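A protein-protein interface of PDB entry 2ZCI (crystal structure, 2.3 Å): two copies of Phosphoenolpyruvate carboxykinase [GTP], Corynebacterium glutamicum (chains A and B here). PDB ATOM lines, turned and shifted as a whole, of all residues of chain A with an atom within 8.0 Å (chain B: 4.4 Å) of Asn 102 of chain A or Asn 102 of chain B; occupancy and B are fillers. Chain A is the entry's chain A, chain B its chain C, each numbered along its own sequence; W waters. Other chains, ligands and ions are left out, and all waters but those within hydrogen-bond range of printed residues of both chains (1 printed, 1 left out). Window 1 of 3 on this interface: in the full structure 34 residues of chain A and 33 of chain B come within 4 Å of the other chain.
The side-chain hydroxyl (OG) of Ser 85 of chain A lies within hydrogen-bond range of the backbone carbonyl oxygen (O) of Asn 101 of chain B (3.0 Å). The backbone carbonyl oxygen (O) of Asn 101 of chain B lies within hydrogen-bond range of the guanidinium group (NH1) of Arg 86 of chain A (2.8 Å). NE of Arg 86 of chain B is in salt-bridge range of OE1 of Glu 94 of chain A (2.5 Å). The backbone carbonyl oxygen (O) of Gly 98 of chain A is in hydrogen-bond range of the guanidinium group (NH2) of Arg 86 of chain B (3.0 Å). O of Asn 101 of chain A lies within hydrogen-bond range of NH1 of Arg 86 of chain B (2.9 Å). The side-chain amide nitrogen (ND2) of Asn 102 of chain A is in hydrogen-bond range of the side-chain amide oxygen (OD1) of Asn 102 of chain B (3.4 Å).
The backbone carbonyl oxygen (O) of Glu 84 of chain A sits close to the side-chain amide oxygen (OD1) of Asn 102 of chain A, at 3.0 Å. The side-chain amide oxygen (OD1) of Asn 102 of chain A sits close to the backbone carbonyl oxygen (O) of Thr 87 of chain A (3.3 Å). The backbone NH (N) of Ile 89 of chain A lies within hydrogen-bond range of the backbone carbonyl oxygen (O) of Asn 102 of chain A. The indole nitrogen (NE1) of Trp 103 of chain A sits at hydrogen-bond distance from the backbone carbonyl oxygen (O) of Ser 91 of chain A (2.7 Å). The backbone NH (N) of Ile 89 of chain B lies within hydrogen-bond range of the backbone carbonyl oxygen (O) of Asn 102 of chain B (3.0 Å). The side-chain amide oxygen of Asn 101 of chain B lies close to the backbone carbonyl oxygen of Ala 97 of chain B, 2.5 Å away.
Water W1 lies within hydrogen-bond range of the backbone carbonyl oxygen of Ser 85 of chain A (2.9 Å), the backbone NH of Trp 103 of chain B (3.2 Å) and the side-chain amide oxygen of Asn 102 of chain B (3.5 Å).
Printed residues of chain B that touch a printed residue of chain A: Ser 85, Arg 86, Phe 88, Ala 97, Asn 101, Asn 102 and Trp 103. Hydrophobic or aromatic side chains of chain B that line the printed part of chain A: Phe 88, Ala 97 and Trp 103. Among the printed residues, 15 pairs touch across the chains.
Among the printed residues, pairs that only touch across the chains: Arg 86 of chain A with Ala 97 of chain B (3.8 Å), Arg 86 of chain A with Trp 103 of chain B (3.8 Å), Phe 88 of chain A with Trp 103 of chain B (3.6 Å), Ala 97 of chain A with Arg 86 of chain B (3.8 Å), Pro 99 of chain A with Ser 85 of chain B (3.6 Å), Asn 101 of chain A with Ser 85 of chain B (3.8 Å), Asn 102 of chain A with Arg 86 of chain B (3.996 Å), Trp 103 of chain A with Arg 86 of chain B (3.5 Å) and Trp 103 of chain A with Phe 88 of chain B (3.4 Å).
Ser 85 of chain A touches Asn 101 of chain B, and with the chains exchanged Asn 101 of chain A touches Ser 85 of chain B. Arg 86 of chain A touches Ala 97 of chain B, and with the chains exchanged Ala 97 of chain A touches Arg 86 of chain B. Asn 102 of chain A touches Arg 86 of chain B, but with the chains exchanged Arg 86 of chain A does not touch Asn 102 of chain B (4.1 Å). Asn 102 of chain A touches its own counterpart, Asn 102 of chain B. 10 positions are printed for both chains. Of the 15 pairs that touch across the chains among the printed residues, 11 have their exchanged pair printed and touching as well.
Ser 91 of chain A touches none of the printed residues of chain B. Printed residues of chain B within 4 Å of Glu 94 of chain A: Arg 86. Printed residues of chain B within 4 Å of Asn 102 of chain A: Arg 86 and Asn 102. Ile 471 of chain A touches none of the printed residues of chain B. Of the printed residues of chain A, Ser 85 of chain B touches Pro 99 and Asn 101. Of chain A, only Asn 102 comes within 4 Å of Asn 102 of chain B. The nearest residue of chain A that does not touch Asn 102 of chain B is Arg 86 of chain A (4.1 Å). The nearest printed residue of chain B that does not touch Ala 97 of chain A is Ser 85 of chain B (8.1 Å).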
ATOM      1  N   VAL A  83     -29.228   3.663  -6.084  1.00  0.00           N
ATOM      2  CA  VAL A  83     -29.455   5.100  -5.894  1.00  0.00           C
ATOM      3  C   VAL A  83     -28.329   5.881  -5.273  1.00  0.00           C
ATOM      4  O   VAL A  83     -28.548   6.894  -4.583  1.00  0.00           O
ATOM      5  CB  VAL A  83     -30.896   5.454  -5.405  1.00  0.00           C
ATOM      6  CG1 VAL A  83     -31.840   5.310  -6.589  1.00  0.00           C
ATOM      7  CG2 VAL A  83     -31.357   4.547  -4.227  1.00  0.00           C
ATOM      8  N   GLU A  84     -27.117   5.433  -5.616  1.00  0.00           N
ATOM      9  CA  GLU A  84     -25.919   6.225  -5.391  1.00  0.00           C
ATOM     10  C   GLU A  84     -25.988   7.628  -5.963  1.00  0.00           C
ATOM     11  O   GLU A  84     -25.590   8.564  -5.315  1.00  0.00           O
ATOM     12  CB  GLU A  84     -24.668   5.477  -5.789  1.00  0.00           C
ATOM     13  CG  GLU A  84     -24.407   4.305  -4.834  1.00  0.00           C
ATOM     14  CD  GLU A  84     -23.466   3.233  -5.419  1.00  0.00           C
ATOM     15  OE1 GLU A  84     -23.947   2.332  -6.162  1.00  0.00           O
ATOM     16  OE2 GLU A  84     -22.241   3.285  -5.101  1.00  0.00           O
ATOM     17  N   SER A  85     -26.593   7.781  -7.104  1.00  0.00           N
ATOM     18  CA  SER A  85     -26.963   9.109  -7.651  1.00  0.00           C
ATOM     19  C   SER A  85     -27.707  10.047  -6.717  1.00  0.00           C
ATOM     20  O   SER A  85     -27.779  11.263  -7.002  1.00  0.00           O
ATOM     21  CB  SER A  85     -27.931   8.921  -8.859  1.00  0.00           C
ATOM     22  OG  SER A  85     -28.146  10.147  -9.594  1.00  0.00           O
ATOM     23  N   ARG A  86     -28.385   9.509  -5.692  1.00  0.00           N
ATOM     24  CA  ARG A  86     -29.275  10.328  -4.841  1.00  0.00           C
ATOM     25  C   ARG A  86     -29.043  10.001  -3.397  1.00  0.00           C
ATOM     26  O   ARG A  86     -29.989   9.902  -2.599  1.00  0.00           O
ATOM     27  CB  ARG A  86     -30.728  10.032  -5.157  1.00  0.00           C
ATOM     28  CG  ARG A  86     -31.265  10.621  -6.461  1.00  0.00           C
ATOM     29  CD  ARG A  86     -31.255  12.140  -6.563  1.00  0.00           C
ATOM     30  NE  ARG A  86     -31.643  12.478  -7.943  1.00  0.00           N
ATOM     31  CZ  ARG A  86     -30.844  12.564  -9.032  1.00  0.00           C
ATOM     32  NH1 ARG A  86     -29.537  12.398  -8.987  1.00  0.00           N
ATOM     33  NH2 ARG A  86     -31.377  12.869 -10.205  1.00  0.00           N
ATOM     34  N   THR A  87     -27.771   9.800  -3.070  1.00  0.00           N
ATOM     35  CA  THR A  87     -27.345   9.463  -1.745  1.00  0.00           C
ATOM     36  C   THR A  87     -26.393  10.638  -1.442  1.00  0.00           C
ATOM     37  O   THR A  87     -25.428  10.877  -2.199  1.00  0.00           O
ATOM     38  CB  THR A  87     -26.700   8.015  -1.737  1.00  0.00           C
ATOM     39  OG1 THR A  87     -27.730   7.095  -2.131  1.00  0.00           O
ATOM     40  CG2 THR A  87     -26.231   7.587  -0.379  1.00  0.00           C
ATOM     41  N   PHE A  88     -26.709  11.377  -0.366  1.00  0.00           N
ATOM     42  CA  PHE A  88     -26.175  12.714  -0.107  1.00  0.00           C
ATOM     43  C   PHE A  88     -25.636  12.767   1.269  1.00  0.00           C
ATOM     44  O   PHE A  88     -26.307  12.369   2.262  1.00  0.00           O
ATOM     45  CB  PHE A  88     -27.301  13.712  -0.105  1.00  0.00           C
ATOM     46  CG  PHE A  88     -27.878  13.971  -1.456  1.00  0.00           C
ATOM     47  CD1 PHE A  88     -28.991  13.281  -1.903  1.00  0.00           C
ATOM     48  CD2 PHE A  88     -27.261  14.855  -2.330  1.00  0.00           C
ATOM     49  CE1 PHE A  88     -29.497  13.481  -3.246  1.00  0.00           C
ATOM     50  CE2 PHE A  88     -27.793  15.079  -3.611  1.00  0.00           C
ATOM     51  CZ  PHE A  88     -28.912  14.391  -4.063  1.00  0.00           C
ATOM     52  N   ILE A  89     -24.429  13.301   1.384  1.00  0.00           N
ATOM     53  CA  ILE A  89     -23.960  13.635   2.640  1.00  0.00           C
ATOM     54  C   ILE A  89     -24.043  15.109   2.661  1.00  0.00           C
ATOM     55  O   ILE A  89     -23.323  15.836   1.920  1.00  0.00           O
ATOM     56  CB  ILE A  89     -22.680  12.865   3.044  1.00  0.00           C
ATOM     57  CG1 ILE A  89     -21.535  13.738   3.190  1.00  0.00           C
ATOM     58  CG2 ILE A  89     -22.459  11.591   2.296  1.00  0.00           C
ATOM     59  CD1 ILE A  89     -21.298  13.991   4.655  1.00  0.00           C
ATOM     60  N   CYS A  90     -25.050  15.536   3.476  1.00  0.00           N
ATOM     61  CA  CYS A  90     -25.459  16.937   3.681  1.00  0.00           C
ATOM     62  C   CYS A  90     -24.784  17.680   4.889  1.00  0.00           C
ATOM     63  O   CYS A  90     -25.418  18.127   5.888  1.00  0.00           O
ATOM     64  CB  CYS A  90     -26.985  17.116   3.632  1.00  0.00           C
ATOM     65  SG  CYS A  90     -27.783  16.741   2.056  1.00  0.00           S
ATOM     66  N   SER A  91     -23.486  17.910   4.735  1.00  0.00           N
ATOM     67  CA  SER A  91     -22.764  18.672   5.733  1.00  0.00           C
ATOM     68  C   SER A  91     -23.082  20.073   5.335  1.00  0.00           C
ATOM     69  O   SER A  91     -23.378  20.309   4.161  1.00  0.00           O
ATOM     70  CB  SER A  91     -21.281  18.425   5.565  1.00  0.00           C
ATOM     71  OG  SER A  91     -21.044  18.114   4.191  1.00  0.00           O
ATOM     72  N   GLU A  94     -19.378  21.860   1.935  1.00  0.00           N
ATOM     73  CA  GLU A  94     -19.399  20.916   0.899  1.00  0.00           C
ATOM     74  C   GLU A  94     -18.118  20.091   0.929  1.00  0.00           C
ATOM     75  O   GLU A  94     -18.047  19.006   0.373  1.00  0.00           O
ATOM     76  CB  GLU A  94     -19.633  21.705  -0.419  1.00  0.00           C
ATOM     77  CG  GLU A  94     -18.450  22.410  -1.091  1.00  0.00           C
ATOM     78  CD  GLU A  94     -17.440  21.413  -1.654  1.00  0.00           C
ATOM     79  OE1 GLU A  94     -17.867  20.382  -2.110  1.00  0.00           O
ATOM     80  OE2 GLU A  94     -16.242  21.619  -1.594  1.00  0.00           O
ATOM     81  N   ALA A  97     -18.153  17.125   2.989  1.00  0.00           N
ATOM     82  CA  ALA A  97     -18.655  15.981   2.276  1.00  0.00           C
ATOM     83  C   ALA A  97     -17.523  15.460   1.412  1.00  0.00           C
ATOM     84  O   ALA A  97     -17.257  14.256   1.449  1.00  0.00           O
ATOM     85  CB  ALA A  97     -19.838  16.325   1.439  1.00  0.00           C
ATOM     86  N   GLY A  98     -16.801  16.352   0.698  1.00  0.00           N
ATOM     87  CA  GLY A  98     -15.549  16.010  -0.022  1.00  0.00           C
ATOM     88  C   GLY A  98     -15.689  15.236  -1.356  1.00  0.00           C
ATOM     89  O   GLY A  98     -16.820  14.938  -1.755  1.00  0.00           O
ATOM     90  N   PRO A  99     -14.542  14.859  -2.014  1.00  0.00           N
ATOM     91  CA  PRO A  99     -14.596  14.443  -3.425  1.00  0.00           C
ATOM     92  C   PRO A  99     -15.122  13.056  -3.746  1.00  0.00           C
ATOM     93  O   PRO A  99     -15.249  12.693  -4.971  1.00  0.00           O
ATOM     94  CB  PRO A  99     -13.110  14.519  -3.873  1.00  0.00           C
ATOM     95  CG  PRO A  99     -12.385  14.029  -2.706  1.00  0.00           C
ATOM     96  CD  PRO A  99     -13.137  14.859  -1.558  1.00  0.00           C
ATOM     97  N   THR A 100     -15.324  12.239  -2.707  1.00  0.00           N
ATOM     98  CA  THR A 100     -15.933  10.928  -2.963  1.00  0.00           C
ATOM     99  C   THR A 100     -17.441  10.937  -2.609  1.00  0.00           C
ATOM    100  O   THR A 100     -18.023   9.924  -2.657  1.00  0.00           O
ATOM    101  CB  THR A 100     -15.183   9.780  -2.205  1.00  0.00           C
ATOM    102  OG1 THR A 100     -15.690   9.646  -0.865  1.00  0.00           O
ATOM    103  CG2 THR A 100     -13.661  10.092  -2.098  1.00  0.00           C
ATOM    104  N   ASN A 101     -18.041  12.087  -2.257  1.00  0.00           N
ATOM    105  CA  ASN A 101     -19.398  12.082  -1.837  1.00  0.00           C
ATOM    106  C   ASN A 101     -20.199  13.061  -2.668  1.00  0.00           C
ATOM    107  O   ASN A 101     -19.638  14.036  -3.169  1.00  0.00           O
ATOM    108  CB  ASN A 101     -19.489  12.449  -0.318  1.00  0.00           C
ATOM    109  CG  ASN A 101     -19.114  11.294   0.627  1.00  0.00           C
ATOM    110  OD1 ASN A 101     -18.657  11.538   1.750  1.00  0.00           O
ATOM    111  ND2 ASN A 101     -19.267  10.042   0.180  1.00  0.00           N
ATOM    112  N   ASN A 102     -21.492  12.762  -2.813  1.00  0.00           N
ATOM    113  CA  ASN A 102     -22.498  13.719  -3.329  1.00  0.00           C
ATOM    114  C   ASN A 102     -22.908  14.674  -2.269  1.00  0.00           C
ATOM    115  O   ASN A 102     -22.994  14.324  -1.102  1.00  0.00           O
ATOM    116  CB  ASN A 102     -23.765  13.012  -3.854  1.00  0.00           C
ATOM    117  CG  ASN A 102     -23.479  12.143  -5.052  1.00  0.00           C
ATOM    118  OD1 ASN A 102     -23.959  11.031  -5.129  1.00  0.00           O
ATOM    119  ND2 ASN A 102     -22.719  12.666  -6.016  1.00  0.00           N
ATOM    120  N   TRP A 103     -23.168  15.905  -2.672  1.00  0.00           N
ATOM    121  CA  TRP A 103     -23.404  16.945  -1.674  1.00  0.00           C
ATOM    122  C   TRP A 103     -24.596  17.790  -2.104  1.00  0.00           C
ATOM    123  O   TRP A 103     -24.888  17.955  -3.320  1.00  0.00           O
ATOM    124  CB  TRP A 103     -22.123  17.775  -1.355  1.00  0.00           C
ATOM    125  CG  TRP A 103     -22.366  18.903  -0.332  1.00  0.00           C
ATOM    126  CD1 TRP A 103     -22.330  18.808   1.012  1.00  0.00           C
ATOM    127  CD2 TRP A 103     -22.757  20.262  -0.621  1.00  0.00           C
ATOM    128  NE1 TRP A 103     -22.632  20.031   1.599  1.00  0.00           N
ATOM    129  CE2 TRP A 103     -22.879  20.943   0.621  1.00  0.00           C
ATOM    130  CE3 TRP A 103     -23.016  20.972  -1.817  1.00  0.00           C
ATOM    131  CZ2 TRP A 103     -23.204  22.305   0.714  1.00  0.00           C
ATOM    132  CZ3 TRP A 103     -23.395  22.316  -1.723  1.00  0.00           C
ATOM    133  CH2 TRP A 103     -23.434  22.976  -0.469  1.00  0.00           C
ATOM    134  N   ALA A 104     -25.341  18.256  -1.099  1.00  0.00           N
ATOM    135  CA  ALA A 104     -26.402  19.196  -1.367  1.00  0.00           C
ATOM    136  C   ALA A 104     -26.673  19.979  -0.078  1.00  0.00           C
ATOM    137  O   ALA A 104     -26.333  19.538   0.970  1.00  0.00           O
ATOM    138  CB  ALA A 104     -27.658  18.475  -2.034  1.00  0.00           C
ATOM    139  N   ILE A 205     -31.659   9.449  -0.207  1.00  0.00           N
ATOM    140  CA  ILE A 205     -31.107   8.926   1.017  1.00  0.00           C
ATOM    141  C   ILE A 205     -30.215  10.117   1.333  1.00  0.00           C
ATOM    142  O   ILE A 205     -29.307  10.431   0.557  1.00  0.00           O
ATOM    143  CB  ILE A 205     -30.253   7.568   0.825  1.00  0.00           C
ATOM    144  CG1 ILE A 205     -31.068   6.367   0.368  1.00  0.00           C
ATOM    145  CG2 ILE A 205     -29.507   7.132   2.106  1.00  0.00           C
ATOM    146  CD1 ILE A 205     -31.558   6.508  -1.102  1.00  0.00           C
ATOM    147  N   GLN A 207     -28.026  11.899   4.554  1.00  0.00           N
ATOM    148  CA  GLN A 207     -27.392  11.826   5.859  1.00  0.00           C
ATOM    149  C   GLN A 207     -27.140  13.286   6.215  1.00  0.00           C
ATOM    150  O   GLN A 207     -26.612  14.013   5.372  1.00  0.00           O
ATOM    151  CB  GLN A 207     -25.989  11.095   5.790  1.00  0.00           C
ATOM    152  CG  GLN A 207     -26.017   9.503   5.773  1.00  0.00           C
ATOM    153  CD  GLN A 207     -26.297   8.826   4.410  1.00  0.00           C
ATOM    154  OE1 GLN A 207     -25.968   9.323   3.288  1.00  0.00           O
ATOM    155  NE2 GLN A 207     -26.922   7.669   4.506  1.00  0.00           N
ATOM    156  N   ILE A 471     -17.948   6.488   3.114  1.00  0.00           N
ATOM    157  CA  ILE A 471     -17.264   7.434   4.019  1.00  0.00           C
ATOM    158  C   ILE A 471     -18.217   8.577   4.293  1.00  0.00           C
ATOM    159  O   ILE A 471     -18.789   9.124   3.366  1.00  0.00           O
ATOM    160  CB  ILE A 471     -15.842   7.919   3.483  1.00  0.00           C
ATOM    161  CG1 ILE A 471     -14.929   6.719   3.201  1.00  0.00           C
ATOM    162  CG2 ILE A 471     -15.154   8.917   4.527  1.00  0.00           C
ATOM    163  CD1 ILE A 471     -13.834   7.022   2.106  1.00  0.00           C
ATOM    164  N   GLU B  84     -16.951  15.397 -11.541  1.00  0.00           N
ATOM    165  CA  GLU B  84     -18.294  14.793 -11.665  1.00  0.00           C
ATOM    166  C   GLU B  84     -19.175  14.969 -10.410  1.00  0.00           C
ATOM    167  O   GLU B  84     -20.322  15.341 -10.501  1.00  0.00           O
ATOM    168  CB  GLU B  84     -18.180  13.263 -12.037  1.00  0.00           C
ATOM    169  CG  GLU B  84     -19.564  12.553 -12.500  1.00  0.00           C
ATOM    170  CD  GLU B  84     -20.091  11.294 -11.624  1.00  0.00           C
ATOM    171  OE1 GLU B  84     -21.271  10.857 -11.872  1.00  0.00           O
ATOM    172  OE2 GLU B  84     -19.376  10.764 -10.734  1.00  0.00           O
ATOM    173  N   SER B  85     -18.644  14.670  -9.237  1.00  0.00           N
ATOM    174  CA  SER B  85     -19.386  14.778  -7.954  1.00  0.00           C
ATOM    175  C   SER B  85     -19.864  16.225  -7.635  1.00  0.00           C
ATOM    176  O   SER B  85     -20.769  16.469  -6.797  1.00  0.00           O
ATOM    177  CB  SER B  85     -18.544  14.221  -6.848  1.00  0.00           C
ATOM    178  OG  SER B  85     -17.349  14.999  -6.715  1.00  0.00           O
ATOM    179  N   ARG B  86     -19.254  17.183  -8.327  1.00  0.00           N
ATOM    180  CA  ARG B  86     -19.684  18.584  -8.190  1.00  0.00           C
ATOM    181  C   ARG B  86     -20.153  19.170  -9.492  1.00  0.00           C
ATOM    182  O   ARG B  86     -19.991  20.358  -9.734  1.00  0.00           O
ATOM    183  CB  ARG B  86     -18.561  19.442  -7.562  1.00  0.00           C
ATOM    184  CG  ARG B  86     -18.150  19.042  -6.117  1.00  0.00           C
ATOM    185  CD  ARG B  86     -19.222  19.387  -5.038  1.00  0.00           C
ATOM    186  NE  ARG B  86     -18.870  18.833  -3.759  1.00  0.00           N
ATOM    187  CZ  ARG B  86     -19.221  17.608  -3.291  1.00  0.00           C
ATOM    188  NH1 ARG B  86     -19.969  16.747  -4.011  1.00  0.00           N
ATOM    189  NH2 ARG B  86     -18.790  17.210  -2.085  1.00  0.00           N
ATOM    190  N   THR B  87     -20.758  18.358 -10.339  1.00  0.00           N
ATOM    191  CA  THR B  87     -21.333  18.857 -11.550  1.00  0.00           C
ATOM    192  C   THR B  87     -22.764  18.465 -11.419  1.00  0.00           C
ATOM    193  O   THR B  87     -23.086  17.290 -11.163  1.00  0.00           O
ATOM    194  CB  THR B  87     -20.705  18.249 -12.810  1.00  0.00           C
ATOM    195  OG1 THR B  87     -19.349  18.666 -12.936  1.00  0.00           O
ATOM    196  CG2 THR B  87     -21.409  18.656 -14.042  1.00  0.00           C
ATOM    197  N   PHE B  88     -23.608  19.485 -11.495  1.00  0.00           N
ATOM    198  CA  PHE B  88     -25.028  19.321 -11.214  1.00  0.00           C
ATOM    199  C   PHE B  88     -25.885  19.763 -12.403  1.00  0.00           C
ATOM    200  O   PHE B  88     -25.607  20.760 -13.067  1.00  0.00           O
ATOM    201  CB  PHE B  88     -25.450  20.144 -10.033  1.00  0.00           C
ATOM    202  CG  PHE B  88     -24.702  19.885  -8.736  1.00  0.00           C
ATOM    203  CD1 PHE B  88     -23.401  20.394  -8.529  1.00  0.00           C
ATOM    204  CD2 PHE B  88     -25.340  19.276  -7.679  1.00  0.00           C
ATOM    205  CE1 PHE B  88     -22.746  20.241  -7.350  1.00  0.00           C
ATOM    206  CE2 PHE B  88     -24.697  19.171  -6.465  1.00  0.00           C
ATOM    207  CZ  PHE B  88     -23.400  19.645  -6.298  1.00  0.00           C
ATOM    208  N   ILE B  89     -26.893  18.965 -12.672  1.00  0.00           N
ATOM    209  CA  ILE B  89     -28.086  19.395 -13.382  1.00  0.00           C
ATOM    210  C   ILE B  89     -29.123  19.853 -12.394  1.00  0.00           C
ATOM    211  O   ILE B  89     -29.772  19.026 -11.721  1.00  0.00           O
ATOM    212  CB  ILE B  89     -28.559  18.276 -14.309  1.00  0.00           C
ATOM    213  CG1 ILE B  89     -27.360  17.868 -15.233  1.00  0.00           C
ATOM    214  CG2 ILE B  89     -29.907  18.579 -15.045  1.00  0.00           C
ATOM    215  CD1 ILE B  89     -27.157  18.775 -16.341  1.00  0.00           C
ATOM    216  N   ALA B  97     -33.500  15.714 -13.920  1.00  0.00           N
ATOM    217  CA  ALA B  97     -32.090  15.325 -13.984  1.00  0.00           C
ATOM    218  C   ALA B  97     -31.937  13.808 -14.266  1.00  0.00           C
ATOM    219  O   ALA B  97     -31.116  13.431 -15.110  1.00  0.00           O
ATOM    220  CB  ALA B  97     -31.390  15.690 -12.788  1.00  0.00           C
ATOM    221  N   ASN B 101     -27.426  11.648 -13.650  1.00  0.00           N
ATOM    222  CA  ASN B 101     -27.070  13.012 -13.336  1.00  0.00           C
ATOM    223  C   ASN B 101     -27.079  13.228 -11.887  1.00  0.00           C
ATOM    224  O   ASN B 101     -27.884  12.646 -11.177  1.00  0.00           O
ATOM    225  CB  ASN B 101     -28.061  14.029 -13.969  1.00  0.00           C
ATOM    226  CG  ASN B 101     -27.980  14.034 -15.500  1.00  0.00           C
ATOM    227  OD1 ASN B 101     -28.999  14.044 -16.238  1.00  0.00           O
ATOM    228  ND2 ASN B 101     -26.766  13.932 -15.985  1.00  0.00           N
ATOM    229  N   ASN B 102     -26.189  14.091 -11.435  1.00  0.00           N
ATOM    230  CA  ASN B 102     -26.320  14.711 -10.138  1.00  0.00           C
ATOM    231  C   ASN B 102     -27.408  15.853 -10.132  1.00  0.00           C
ATOM    232  O   ASN B 102     -27.679  16.503 -11.193  1.00  0.00           O
ATOM    233  CB  ASN B 102     -24.941  15.192  -9.679  1.00  0.00           C
ATOM    234  CG  ASN B 102     -23.918  14.056  -9.511  1.00  0.00           C
ATOM    235  OD1 ASN B 102     -24.220  12.887  -9.109  1.00  0.00           O
ATOM    236  ND2 ASN B 102     -22.649  14.423  -9.762  1.00  0.00           N
ATOM    237  N   TRP B 103     -28.006  16.083  -8.958  1.00  0.00           N
ATOM    238  CA  TRP B 103     -29.054  17.064  -8.791  1.00  0.00           C
ATOM    239  C   TRP B 103     -28.967  17.697  -7.425  1.00  0.00           C
ATOM    240  O   TRP B 103     -28.465  17.120  -6.446  1.00  0.00           O
ATOM    241  CB  TRP B 103     -30.420  16.347  -8.914  1.00  0.00           C
ATOM    242  CG  TRP B 103     -31.606  17.324  -8.719  1.00  0.00           C
ATOM    243  CD1 TRP B 103     -32.135  18.084  -9.652  1.00  0.00           C
ATOM    244  CD2 TRP B 103     -32.308  17.624  -7.497  1.00  0.00           C
ATOM    245  NE1 TRP B 103     -33.138  18.837  -9.132  1.00  0.00           N
ATOM    246  CE2 TRP B 103     -33.271  18.583  -7.806  1.00  0.00           C
ATOM    247  CE3 TRP B 103     -32.180  17.201  -6.185  1.00  0.00           C
ATOM    248  CZ2 TRP B 103     -34.142  19.157  -6.845  1.00  0.00           C
ATOM    249  CZ3 TRP B 103     -33.050  17.717  -5.261  1.00  0.00           C
ATOM    250  CH2 TRP B 103     -34.016  18.717  -5.605  1.00  0.00           C
HETATM  251  O   HOH W   1     -26.723  13.998  -6.955  1.00  0.00           O
